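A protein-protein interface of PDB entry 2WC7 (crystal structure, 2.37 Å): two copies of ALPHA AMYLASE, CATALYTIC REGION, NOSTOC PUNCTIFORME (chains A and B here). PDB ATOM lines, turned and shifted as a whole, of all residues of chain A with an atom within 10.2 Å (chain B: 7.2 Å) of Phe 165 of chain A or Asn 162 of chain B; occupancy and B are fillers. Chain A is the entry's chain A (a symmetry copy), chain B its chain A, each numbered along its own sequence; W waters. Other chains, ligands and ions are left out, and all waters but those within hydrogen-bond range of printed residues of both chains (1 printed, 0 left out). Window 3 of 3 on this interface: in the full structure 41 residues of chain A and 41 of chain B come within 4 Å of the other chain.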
ATOM      1  N   ARG A 130     -13.910   1.947  12.634  1.00  0.00           N
ATOM      2  CA  ARG A 130     -15.119   1.195  12.970  1.00  0.00           C
ATOM      3  C   ARG A 130     -15.613   1.542  14.372  1.00  0.00           C
ATOM      4  O   ARG A 130     -16.737   1.202  14.744  1.00  0.00           O
ATOM      5  CB  ARG A 130     -14.867  -0.314  12.902  1.00  0.00           C
ATOM      6  CG  ARG A 130     -14.617  -0.867  11.518  1.00  0.00           C
ATOM      7  CD  ARG A 130     -13.200  -1.349  11.442  1.00  0.00           C
ATOM      8  NE  ARG A 130     -13.073  -2.732  11.009  1.00  0.00           N
ATOM      9  CZ  ARG A 130     -11.954  -3.434  11.134  1.00  0.00           C
ATOM     10  NH1 ARG A 130     -10.884  -2.880  11.682  1.00  0.00           N
ATOM     11  NH2 ARG A 130     -11.894  -4.684  10.703  1.00  0.00           N
ATOM     12  N   LEU A 139     -23.139   0.199  12.845  1.00  0.00           N
ATOM     13  CA  LEU A 139     -22.834  -1.221  12.969  1.00  0.00           C
ATOM     14  C   LEU A 139     -23.776  -1.890  13.954  1.00  0.00           C
ATOM     15  O   LEU A 139     -24.061  -3.080  13.831  1.00  0.00           O
ATOM     16  CB  LEU A 139     -21.395  -1.441  13.445  1.00  0.00           C
ATOM     17  CG  LEU A 139     -20.255  -1.078  12.488  1.00  0.00           C
ATOM     18  CD1 LEU A 139     -18.919  -1.485  13.121  1.00  0.00           C
ATOM     19  CD2 LEU A 139     -20.459  -1.780  11.154  1.00  0.00           C
ATOM     20  N   GLU A 140     -24.262  -1.122  14.928  1.00  0.00           N
ATOM     21  CA  GLU A 140     -25.162  -1.647  15.958  1.00  0.00           C
ATOM     22  C   GLU A 140     -26.627  -1.646  15.529  1.00  0.00           C
ATOM     23  O   GLU A 140     -27.373  -2.558  15.866  1.00  0.00           O
ATOM     24  CB  GLU A 140     -25.037  -0.823  17.256  1.00  0.00           C
ATOM     25  CG  GLU A 140     -23.619  -0.670  17.806  1.00  0.00           C
ATOM     26  CD  GLU A 140     -23.130  -1.881  18.583  1.00  0.00           C
ATOM     27  OE1 GLU A 140     -21.991  -2.326  18.334  1.00  0.00           O
ATOM     28  OE2 GLU A 140     -23.872  -2.377  19.456  1.00  0.00           O
ATOM     29  N   GLY A 155     -24.885  -1.887   0.640  1.00  0.00           N
ATOM     30  CA  GLY A 155     -25.885  -2.929   0.794  1.00  0.00           C
ATOM     31  C   GLY A 155     -25.850  -3.547   2.172  1.00  0.00           C
ATOM     32  O   GLY A 155     -24.926  -3.282   2.941  1.00  0.00           O
ATOM     33  N   TRP A 156     -26.847  -4.368   2.495  1.00  0.00           N
ATOM     34  CA  TRP A 156     -26.903  -5.015   3.802  1.00  0.00           C
ATOM     35  C   TRP A 156     -26.836  -6.528   3.678  1.00  0.00           C
ATOM     36  O   TRP A 156     -27.251  -7.097   2.665  1.00  0.00           O
ATOM     37  CB  TRP A 156     -28.190  -4.643   4.532  1.00  0.00           C
ATOM     38  CG  TRP A 156     -28.479  -3.187   4.531  1.00  0.00           C
ATOM     39  CD1 TRP A 156     -29.284  -2.513   3.662  1.00  0.00           C
ATOM     40  CD2 TRP A 156     -27.962  -2.213   5.441  1.00  0.00           C
ATOM     41  NE1 TRP A 156     -29.304  -1.177   3.977  1.00  0.00           N
ATOM     42  CE2 TRP A 156     -28.501  -0.964   5.068  1.00  0.00           C
ATOM     43  CE3 TRP A 156     -27.093  -2.273   6.540  1.00  0.00           C
ATOM     44  CZ2 TRP A 156     -28.202   0.218   5.754  1.00  0.00           C
ATOM     45  CZ3 TRP A 156     -26.795  -1.096   7.223  1.00  0.00           C
ATOM     46  CH2 TRP A 156     -27.350   0.130   6.826  1.00  0.00           C
ATOM     47  N   PRO A 157     -26.315  -7.205   4.713  1.00  0.00           N
ATOM     48  CA  PRO A 157     -25.811  -6.577   5.938  1.00  0.00           C
ATOM     49  C   PRO A 157     -24.345  -6.196   5.787  1.00  0.00           C
ATOM     50  O   PRO A 157     -23.678  -6.612   4.839  1.00  0.00           O
ATOM     51  CB  PRO A 157     -26.006  -7.667   6.978  1.00  0.00           C
ATOM     52  CG  PRO A 157     -25.648  -8.890   6.200  1.00  0.00           C
ATOM     53  CD  PRO A 157     -26.391  -8.668   4.882  1.00  0.00           C
ATOM     54  N   LEU A 158     -23.846  -5.408   6.730  1.00  0.00           N
ATOM     55  CA  LEU A 158     -22.459  -4.985   6.693  1.00  0.00           C
ATOM     56  C   LEU A 158     -21.603  -6.053   7.352  1.00  0.00           C
ATOM     57  O   LEU A 158     -22.077  -6.797   8.211  1.00  0.00           O
ATOM     58  CB  LEU A 158     -22.297  -3.661   7.436  1.00  0.00           C
ATOM     59  CG  LEU A 158     -23.192  -2.504   6.979  1.00  0.00           C
ATOM     60  CD1 LEU A 158     -22.905  -1.275   7.823  1.00  0.00           C
ATOM     61  CD2 LEU A 158     -22.949  -2.202   5.508  1.00  0.00           C
ATOM     62  N   SER A 159     -20.346  -6.145   6.938  1.00  0.00           N
ATOM     63  CA  SER A 159     -19.438  -7.112   7.536  1.00  0.00           C
ATOM     64  C   SER A 159     -18.189  -6.343   7.946  1.00  0.00           C
ATOM     65  O   SER A 159     -17.159  -6.371   7.268  1.00  0.00           O
ATOM     66  CB  SER A 159     -19.086  -8.220   6.548  1.00  0.00           C
ATOM     67  OG  SER A 159     -18.387  -9.258   7.213  1.00  0.00           O
ATOM     68  N   PRO A 160     -18.272  -5.637   9.075  1.00  0.00           N
ATOM     69  CA  PRO A 160     -17.159  -4.842   9.589  1.00  0.00           C
ATOM     70  C   PRO A 160     -15.849  -5.573   9.851  1.00  0.00           C
ATOM     71  O   PRO A 160     -14.789  -5.099   9.433  1.00  0.00           O
ATOM     72  CB  PRO A 160     -17.744  -4.214  10.851  1.00  0.00           C
ATOM     73  CG  PRO A 160     -18.760  -5.225  11.291  1.00  0.00           C
ATOM     74  CD  PRO A 160     -19.419  -5.588   9.998  1.00  0.00           C
ATOM     75  N   TYR A 161     -15.907  -6.721  10.523  1.00  0.00           N
ATOM     76  CA  TYR A 161     -14.679  -7.440  10.843  1.00  0.00           C
ATOM     77  C   TYR A 161     -14.454  -8.804  10.216  1.00  0.00           C
ATOM     78  O   TYR A 161     -13.356  -9.351  10.319  1.00  0.00           O
ATOM     79  CB  TYR A 161     -14.534  -7.579  12.360  1.00  0.00           C
ATOM     80  CG  TYR A 161     -14.374  -6.266  13.092  1.00  0.00           C
ATOM     81  CD1 TYR A 161     -15.481  -5.473  13.394  1.00  0.00           C
ATOM     82  CD2 TYR A 161     -13.115  -5.821  13.492  1.00  0.00           C
ATOM     83  CE1 TYR A 161     -15.335  -4.270  14.084  1.00  0.00           C
ATOM     84  CE2 TYR A 161     -12.960  -4.619  14.177  1.00  0.00           C
ATOM     85  CZ  TYR A 161     -14.070  -3.851  14.471  1.00  0.00           C
ATOM     86  OH  TYR A 161     -13.916  -2.664  15.149  1.00  0.00           O
ATOM     87  N   ASN A 162     -15.466  -9.373   9.574  1.00  0.00           N
ATOM     88  CA  ASN A 162     -15.270 -10.689   8.982  1.00  0.00           C
ATOM     89  C   ASN A 162     -14.952 -10.595   7.495  1.00  0.00           C
ATOM     90  O   ASN A 162     -15.845 -10.449   6.661  1.00  0.00           O
ATOM     91  CB  ASN A 162     -16.498 -11.570   9.217  1.00  0.00           C
ATOM     92  CG  ASN A 162     -16.163 -13.046   9.165  1.00  0.00           C
ATOM     93  OD1 ASN A 162     -16.646 -13.838   9.980  1.00  0.00           O
ATOM     94  ND2 ASN A 162     -15.331 -13.428   8.201  1.00  0.00           N
ATOM     95  N   GLY A 163     -13.662 -10.693   7.181  1.00  0.00           N
ATOM     96  CA  GLY A 163     -13.200 -10.590   5.809  1.00  0.00           C
ATOM     97  C   GLY A 163     -13.683 -11.652   4.841  1.00  0.00           C
ATOM     98  O   GLY A 163     -13.418 -11.566   3.641  1.00  0.00           O
ATOM     99  N   GLU A 164     -14.388 -12.656   5.352  1.00  0.00           N
ATOM    100  CA  GLU A 164     -14.891 -13.725   4.506  1.00  0.00           C
ATOM    101  C   GLU A 164     -16.161 -13.299   3.774  1.00  0.00           C
ATOM    102  O   GLU A 164     -16.606 -13.976   2.849  1.00  0.00           O
ATOM    103  CB  GLU A 164     -15.169 -14.967   5.350  1.00  0.00           C
ATOM    104  CG  GLU A 164     -15.506 -16.205   4.539  1.00  0.00           C
ATOM    105  CD  GLU A 164     -15.869 -17.400   5.408  1.00  0.00           C
ATOM    106  OE1 GLU A 164     -16.155 -18.479   4.839  1.00  0.00           O
ATOM    107  OE2 GLU A 164     -15.873 -17.259   6.655  1.00  0.00           O
ATOM    108  N   PHE A 165     -16.743 -12.177   4.188  1.00  0.00           N
ATOM    109  CA  PHE A 165     -17.964 -11.665   3.568  1.00  0.00           C
ATOM    110  C   PHE A 165     -17.722 -10.226   3.124  1.00  0.00           C
ATOM    111  O   PHE A 165     -16.866  -9.543   3.668  1.00  0.00           O
ATOM    112  CB  PHE A 165     -19.133 -11.684   4.562  1.00  0.00           C
ATOM    113  CG  PHE A 165     -19.330 -13.005   5.259  1.00  0.00           C
ATOM    114  CD1 PHE A 165     -18.392 -13.473   6.183  1.00  0.00           C
ATOM    115  CD2 PHE A 165     -20.462 -13.777   5.007  1.00  0.00           C
ATOM    116  CE1 PHE A 165     -18.583 -14.691   6.844  1.00  0.00           C
ATOM    117  CE2 PHE A 165     -20.662 -14.994   5.662  1.00  0.00           C
ATOM    118  CZ  PHE A 165     -19.720 -15.451   6.583  1.00  0.00           C
ATOM    119  N   PRO A 166     -18.486  -9.743   2.139  1.00  0.00           N
ATOM    120  CA  PRO A 166     -18.309  -8.368   1.661  1.00  0.00           C
ATOM    121  C   PRO A 166     -18.659  -7.318   2.720  1.00  0.00           C
ATOM    122  O   PRO A 166     -19.715  -7.385   3.349  1.00  0.00           O
ATOM    123  CB  PRO A 166     -19.239  -8.309   0.454  1.00  0.00           C
ATOM    124  CG  PRO A 166     -20.372  -9.211   0.880  1.00  0.00           C
ATOM    125  CD  PRO A 166     -19.639 -10.390   1.485  1.00  0.00           C
ATOM    126  N   ALA A 167     -17.768  -6.351   2.913  1.00  0.00           N
ATOM    127  CA  ALA A 167     -17.993  -5.298   3.900  1.00  0.00           C
ATOM    128  C   ALA A 167     -19.327  -4.594   3.657  1.00  0.00           C
ATOM    129  O   ALA A 167     -20.091  -4.339   4.592  1.00  0.00           O
ATOM    130  CB  ALA A 167     -16.855  -4.286   3.854  1.00  0.00           C
ATOM    131  N   ASN A 168     -19.592  -4.288   2.393  1.00  0.00           N
ATOM    132  CA  ASN A 168     -20.813  -3.612   1.980  1.00  0.00           C
ATOM    133  C   ASN A 168     -20.876  -2.127   2.302  1.00  0.00           C
ATOM    134  O   ASN A 168     -21.953  -1.527   2.295  1.00  0.00           O
ATOM    135  CB  ASN A 168     -22.045  -4.320   2.538  1.00  0.00           C
ATOM    136  CG  ASN A 168     -22.545  -5.405   1.609  1.00  0.00           C
ATOM    137  OD1 ASN A 168     -22.580  -5.216   0.394  1.00  0.00           O
ATOM    138  ND2 ASN A 168     -22.943  -6.543   2.170  1.00  0.00           N
ATOM    139  N   TYR A 169     -19.711  -1.546   2.578  1.00  0.00           N
ATOM    140  CA  TYR A 169     -19.590  -0.118   2.853  1.00  0.00           C
ATOM    141  C   TYR A 169     -18.204   0.319   2.368  1.00  0.00           C
ATOM    142  O   TYR A 169     -17.234  -0.425   2.491  1.00  0.00           O
ATOM    143  CB  TYR A 169     -19.812   0.177   4.350  1.00  0.00           C
ATOM    144  CG  TYR A 169     -18.779  -0.367   5.313  1.00  0.00           C
ATOM    145  CD1 TYR A 169     -17.541   0.255   5.461  1.00  0.00           C
ATOM    146  CD2 TYR A 169     -19.055  -1.485   6.111  1.00  0.00           C
ATOM    147  CE1 TYR A 169     -16.598  -0.213   6.381  1.00  0.00           C
ATOM    148  CE2 TYR A 169     -18.118  -1.965   7.036  1.00  0.00           C
ATOM    149  CZ  TYR A 169     -16.890  -1.321   7.167  1.00  0.00           C
ATOM    150  OH  TYR A 169     -15.956  -1.762   8.079  1.00  0.00           O
ATOM    151  N   GLY A 174     -10.379   0.674  -0.298  1.00  0.00           N
ATOM    152  CA  GLY A 174     -11.039  -0.613  -0.162  1.00  0.00           C
ATOM    153  C   GLY A 174     -10.781  -1.337   1.148  1.00  0.00           C
ATOM    154  O   GLY A 174     -10.970  -2.551   1.237  1.00  0.00           O
ATOM    155  N   ARG A 176     -11.786  -1.994   5.030  1.00  0.00           N
ATOM    156  CA  ARG A 176     -12.931  -1.891   5.939  1.00  0.00           C
ATOM    157  C   ARG A 176     -12.685  -1.072   7.199  1.00  0.00           C
ATOM    158  O   ARG A 176     -13.616  -0.506   7.771  1.00  0.00           O
ATOM    159  CB  ARG A 176     -13.381  -3.278   6.377  1.00  0.00           C
ATOM    160  CG  ARG A 176     -13.478  -4.264   5.254  1.00  0.00           C
ATOM    161  CD  ARG A 176     -13.965  -5.588   5.771  1.00  0.00           C
ATOM    162  NE  ARG A 176     -14.038  -6.563   4.695  1.00  0.00           N
ATOM    163  CZ  ARG A 176     -14.693  -7.712   4.783  1.00  0.00           C
ATOM    164  NH1 ARG A 176     -15.332  -8.024   5.902  1.00  0.00           N
ATOM    165  NH2 ARG A 176     -14.696  -8.550   3.759  1.00  0.00           N
ATOM    166  N   ARG B 130     -19.269  -2.416  21.944  1.00  0.00           N
ATOM    167  CA  ARG B 130     -18.219  -2.780  20.993  1.00  0.00           C
ATOM    168  C   ARG B 130     -17.500  -1.542  20.463  1.00  0.00           C
ATOM    169  O   ARG B 130     -16.438  -1.648  19.846  1.00  0.00           O
ATOM    170  CB  ARG B 130     -18.795  -3.554  19.805  1.00  0.00           C
ATOM    171  CG  ARG B 130     -19.320  -4.936  20.125  1.00  0.00           C
ATOM    172  CD  ARG B 130     -20.806  -4.940  19.932  1.00  0.00           C
ATOM    173  NE  ARG B 130     -21.277  -5.982  19.032  1.00  0.00           N
ATOM    174  CZ  ARG B 130     -22.499  -5.996  18.512  1.00  0.00           C
ATOM    175  NH1 ARG B 130     -23.352  -5.026  18.802  1.00  0.00           N
ATOM    176  NH2 ARG B 130     -22.876  -6.982  17.713  1.00  0.00           N
ATOM    177  N   SER B 159     -15.440 -12.677  17.540  1.00  0.00           N
ATOM    178  CA  SER B 159     -16.459 -12.478  16.518  1.00  0.00           C
ATOM    179  C   SER B 159     -17.456 -11.476  17.083  1.00  0.00           C
ATOM    180  O   SER B 159     -18.540 -11.833  17.549  1.00  0.00           O
ATOM    181  CB  SER B 159     -17.154 -13.792  16.175  1.00  0.00           C
ATOM    182  OG  SER B 159     -17.976 -13.619  15.032  1.00  0.00           O
ATOM    183  N   PRO B 160     -17.090 -10.193  17.049  1.00  0.00           N
ATOM    184  CA  PRO B 160     -17.938  -9.121  17.563  1.00  0.00           C
ATOM    185  C   PRO B 160     -19.333  -8.995  16.968  1.00  0.00           C
ATOM    186  O   PRO B 160     -20.309  -8.872  17.714  1.00  0.00           O
ATOM    187  CB  PRO B 160     -17.086  -7.874  17.332  1.00  0.00           C
ATOM    188  CG  PRO B 160     -16.267  -8.244  16.132  1.00  0.00           C
ATOM    189  CD  PRO B 160     -15.858  -9.647  16.454  1.00  0.00           C
ATOM    190  N   TYR B 161     -19.444  -9.035  15.642  1.00  0.00           N
ATOM    191  CA  TYR B 161     -20.751  -8.872  15.015  1.00  0.00           C
ATOM    192  C   TYR B 161     -21.337 -10.044  14.247  1.00  0.00           C
ATOM    193  O   TYR B 161     -22.507 -10.003  13.866  1.00  0.00           O
ATOM    194  CB  TYR B 161     -20.743  -7.651  14.095  1.00  0.00           C
ATOM    195  CG  TYR B 161     -20.529  -6.336  14.808  1.00  0.00           C
ATOM    196  CD1 TYR B 161     -19.251  -5.916  15.173  1.00  0.00           C
ATOM    197  CD2 TYR B 161     -21.607  -5.505  15.111  1.00  0.00           C
ATOM    198  CE1 TYR B 161     -19.052  -4.696  15.818  1.00  0.00           C
ATOM    199  CE2 TYR B 161     -21.418  -4.287  15.758  1.00  0.00           C
ATOM    200  CZ  TYR B 161     -20.142  -3.888  16.107  1.00  0.00           C
ATOM    201  OH  TYR B 161     -19.956  -2.684  16.744  1.00  0.00           O
ATOM    202  N   ASN B 162     -20.554 -11.086  14.002  1.00  0.00           N
ATOM    203  CA  ASN B 162     -21.097 -12.211  13.251  1.00  0.00           C
ATOM    204  C   ASN B 162     -21.560 -13.331  14.173  1.00  0.00           C
ATOM    205  O   ASN B 162     -20.762 -14.142  14.641  1.00  0.00           O
ATOM    206  CB  ASN B 162     -20.067 -12.730  12.246  1.00  0.00           C
ATOM    207  CG  ASN B 162     -20.715 -13.457  11.085  1.00  0.00           C
ATOM    208  OD1 ASN B 162     -20.321 -13.288   9.928  1.00  0.00           O
ATOM    209  ND2 ASN B 162     -21.718 -14.274  11.389  1.00  0.00           N
ATOM    210  N   GLY B 163     -22.869 -13.365  14.415  1.00  0.00           N
ATOM    211  CA  GLY B 163     -23.457 -14.355  15.299  1.00  0.00           C
ATOM    212  C   GLY B 163     -23.331 -15.807  14.882  1.00  0.00           C
ATOM    213  O   GLY B 163     -23.712 -16.704  15.637  1.00  0.00           O
ATOM    214  N   GLU B 164     -22.803 -16.048  13.688  1.00  0.00           N
ATOM    215  CA  GLU B 164     -22.645 -17.406  13.197  1.00  0.00           C
ATOM    216  C   GLU B 164     -21.409 -18.071  13.798  1.00  0.00           C
ATOM    217  O   GLU B 164     -21.232 -19.282  13.684  1.00  0.00           O
ATOM    218  CB  GLU B 164     -22.543 -17.400  11.673  1.00  0.00           C
ATOM    219  CG  GLU B 164     -22.578 -18.781  11.043  1.00  0.00           C
ATOM    220  CD  GLU B 164     -22.379 -18.746   9.536  1.00  0.00           C
ATOM    221  OE1 GLU B 164     -22.401 -19.833   8.912  1.00  0.00           O
ATOM    222  OE2 GLU B 164     -22.198 -17.638   8.976  1.00  0.00           O
ATOM    223  N   PHE B 165     -20.555 -17.276  14.438  1.00  0.00           N
ATOM    224  CA  PHE B 165     -19.334 -17.793  15.057  1.00  0.00           C
ATOM    225  C   PHE B 165     -19.313 -17.374  16.522  1.00  0.00           C
ATOM    226  O   PHE B 165     -19.931 -16.387  16.897  1.00  0.00           O
ATOM    227  CB  PHE B 165     -18.088 -17.226  14.363  1.00  0.00           C
ATOM    228  CG  PHE B 165     -18.098 -17.365  12.863  1.00  0.00           C
ATOM    229  CD1 PHE B 165     -18.998 -16.635  12.084  1.00  0.00           C
ATOM    230  CD2 PHE B 165     -17.196 -18.213  12.224  1.00  0.00           C
ATOM    231  CE1 PHE B 165     -18.997 -16.748  10.690  1.00  0.00           C
ATOM    232  CE2 PHE B 165     -17.187 -18.333  10.833  1.00  0.00           C
ATOM    233  CZ  PHE B 165     -18.089 -17.599  10.064  1.00  0.00           C
ATOM    234  N   PRO B 166     -18.584 -18.110  17.369  1.00  0.00           N
ATOM    235  CA  PRO B 166     -18.517 -17.767  18.793  1.00  0.00           C
ATOM    236  C   PRO B 166     -17.827 -16.423  19.050  1.00  0.00           C
ATOM    237  O   PRO B 166     -16.744 -16.162  18.529  1.00  0.00           O
ATOM    238  CB  PRO B 166     -17.745 -18.940  19.386  1.00  0.00           C
ATOM    239  CG  PRO B 166     -16.790 -19.291  18.270  1.00  0.00           C
ATOM    240  CD  PRO B 166     -17.683 -19.232  17.048  1.00  0.00           C
ATOM    241  N   ALA B 167     -18.460 -15.576  19.855  1.00  0.00           N
ATOM    242  CA  ALA B 167     -17.899 -14.265  20.170  1.00  0.00           C
ATOM    243  C   ALA B 167     -16.484 -14.394  20.729  1.00  0.00           C
ATOM    244  O   ALA B 167     -15.578 -13.649  20.345  1.00  0.00           O
ATOM    245  CB  ALA B 167     -18.790 -13.541  21.172  1.00  0.00           C
ATOM    246  N   ARG B 176     -23.074 -10.301  23.039  1.00  0.00           N
ATOM    247  CA  ARG B 176     -21.834  -9.738  22.497  1.00  0.00           C
ATOM    248  C   ARG B 176     -21.747  -8.218  22.524  1.00  0.00           C
ATOM    249  O   ARG B 176     -20.656  -7.653  22.575  1.00  0.00           O
ATOM    250  CB  ARG B 176     -21.644 -10.180  21.052  1.00  0.00           C
ATOM    251  CG  ARG B 176     -21.894 -11.640  20.830  1.00  0.00           C
ATOM    252  CD  ARG B 176     -21.645 -11.992  19.390  1.00  0.00           C
ATOM    253  NE  ARG B 176     -21.911 -13.402  19.154  1.00  0.00           N
ATOM    254  CZ  ARG B 176     -21.513 -14.056  18.073  1.00  0.00           C
ATOM    255  NH1 ARG B 176     -20.828 -13.423  17.131  1.00  0.00           N
ATOM    256  NH2 ARG B 176     -21.811 -15.338  17.930  1.00  0.00           N
HETATM  257  O   HOH W   1     -22.324  -2.939  21.636  1.00  0.00           O
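The guanidinium group (NH2) of Arg 130 of chain B lies within hydrogen-bond range of the backbone carbonyl oxygen (O) of Pro 160 of chain B, 3.2 Å away. N of Glu 164 of chain B sits close to ND2 of Asn 162 of chain B, at 3.1 Å. The backbone carbonyl oxygen (O) of Phe 165 of chain B sits close to the guanidinium group (NH1) of Arg 176 of chain B (3.1 Å). NH2 of Arg 130 of chain A sits at hydrogen-bond distance from O of Pro 160 of chain A (3.2 Å). The side-chain amide nitrogen (ND2) of Asn 162 of chain A lies close to the backbone NH (N) of Glu 164 of chain A, at 3.1 Å. The backbone carbonyl oxygen (O) of Asn 162 of chain A sits at hydrogen-bond distance from the guanidinium group (NH1) of Arg 176 of chain A, 2.6 Å away.
Water W1 bridges OE2 of Glu 140 of chain A (2.7 Å) and N of Arg 130 of chain B (3.1 Å).
Of the 11 printed residues of chain B, 5 touch a printed residue of chain A. Hydrophobic or aromatic side chains of chain B within 4 Å of the printed part of chain A: Pro 160, Tyr 161 and Phe 165. Among the printed residues, 8 pairs touch across the chains.
Pro 160 of chain A touches Tyr 161 of chain B, and with the chains exchanged Tyr 161 of chain A touches Pro 160 of chain B. Asn 162 of chain A touches its own counterpart, Asn 162 of chain B. Asn 162 of chain A touches Phe 165 of chain B, and with the chains exchanged Phe 165 of chain A touches Asn 162 of chain B. Positions printed for both chains: 130, 159, 160, 161, 162, 163, 164, 165, 166, 167 and 176.
Of chain A, only Asn 162 (3.7 Å) and Phe 165 (3.8 Å) come within 4 Å of Asn 162 of chain B. Of chain A, only Tyr 161 (3.97 Å) comes within 4 Å of Pro 160 of chain B. Of the printed residues of chain B, Glu 140 of chain A touches Arg 130 (2.8 Å) and Tyr 161 (2.6 Å). Of the printed residues of chain B, Asn 162 of chain A touches Asn 162 and Phe 165. Of the printed residues of chain A, Arg 130 of chain B touches Glu 140. Leu 158 of chain A touches none of the printed residues of chain B. Trp 156 of chain A touches none of the printed residues of chain B.
Among the printed residues, pairs that only touch across the chains: Leu 139 of chain A with Tyr 161 of chain B, Asn 162 of chain A with Asn 162 of chain B, Asn 162 of chain A with Phe 165 of chain B, Phe 165 of chain A with Asn 162 of chain B, Pro 160 of chain A with Tyr 161 of chain B and Tyr 161 of chain A with Pro 160 of chain B.
OE2 of Glu 140 of chain A is in salt-bridge range of NH1 of Arg 130 of chain B, 2.8 Å away. OH of Tyr 161 of chain B lies within hydrogen-bond range of OE1 of Glu 140 of chain A (2.6 Å).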
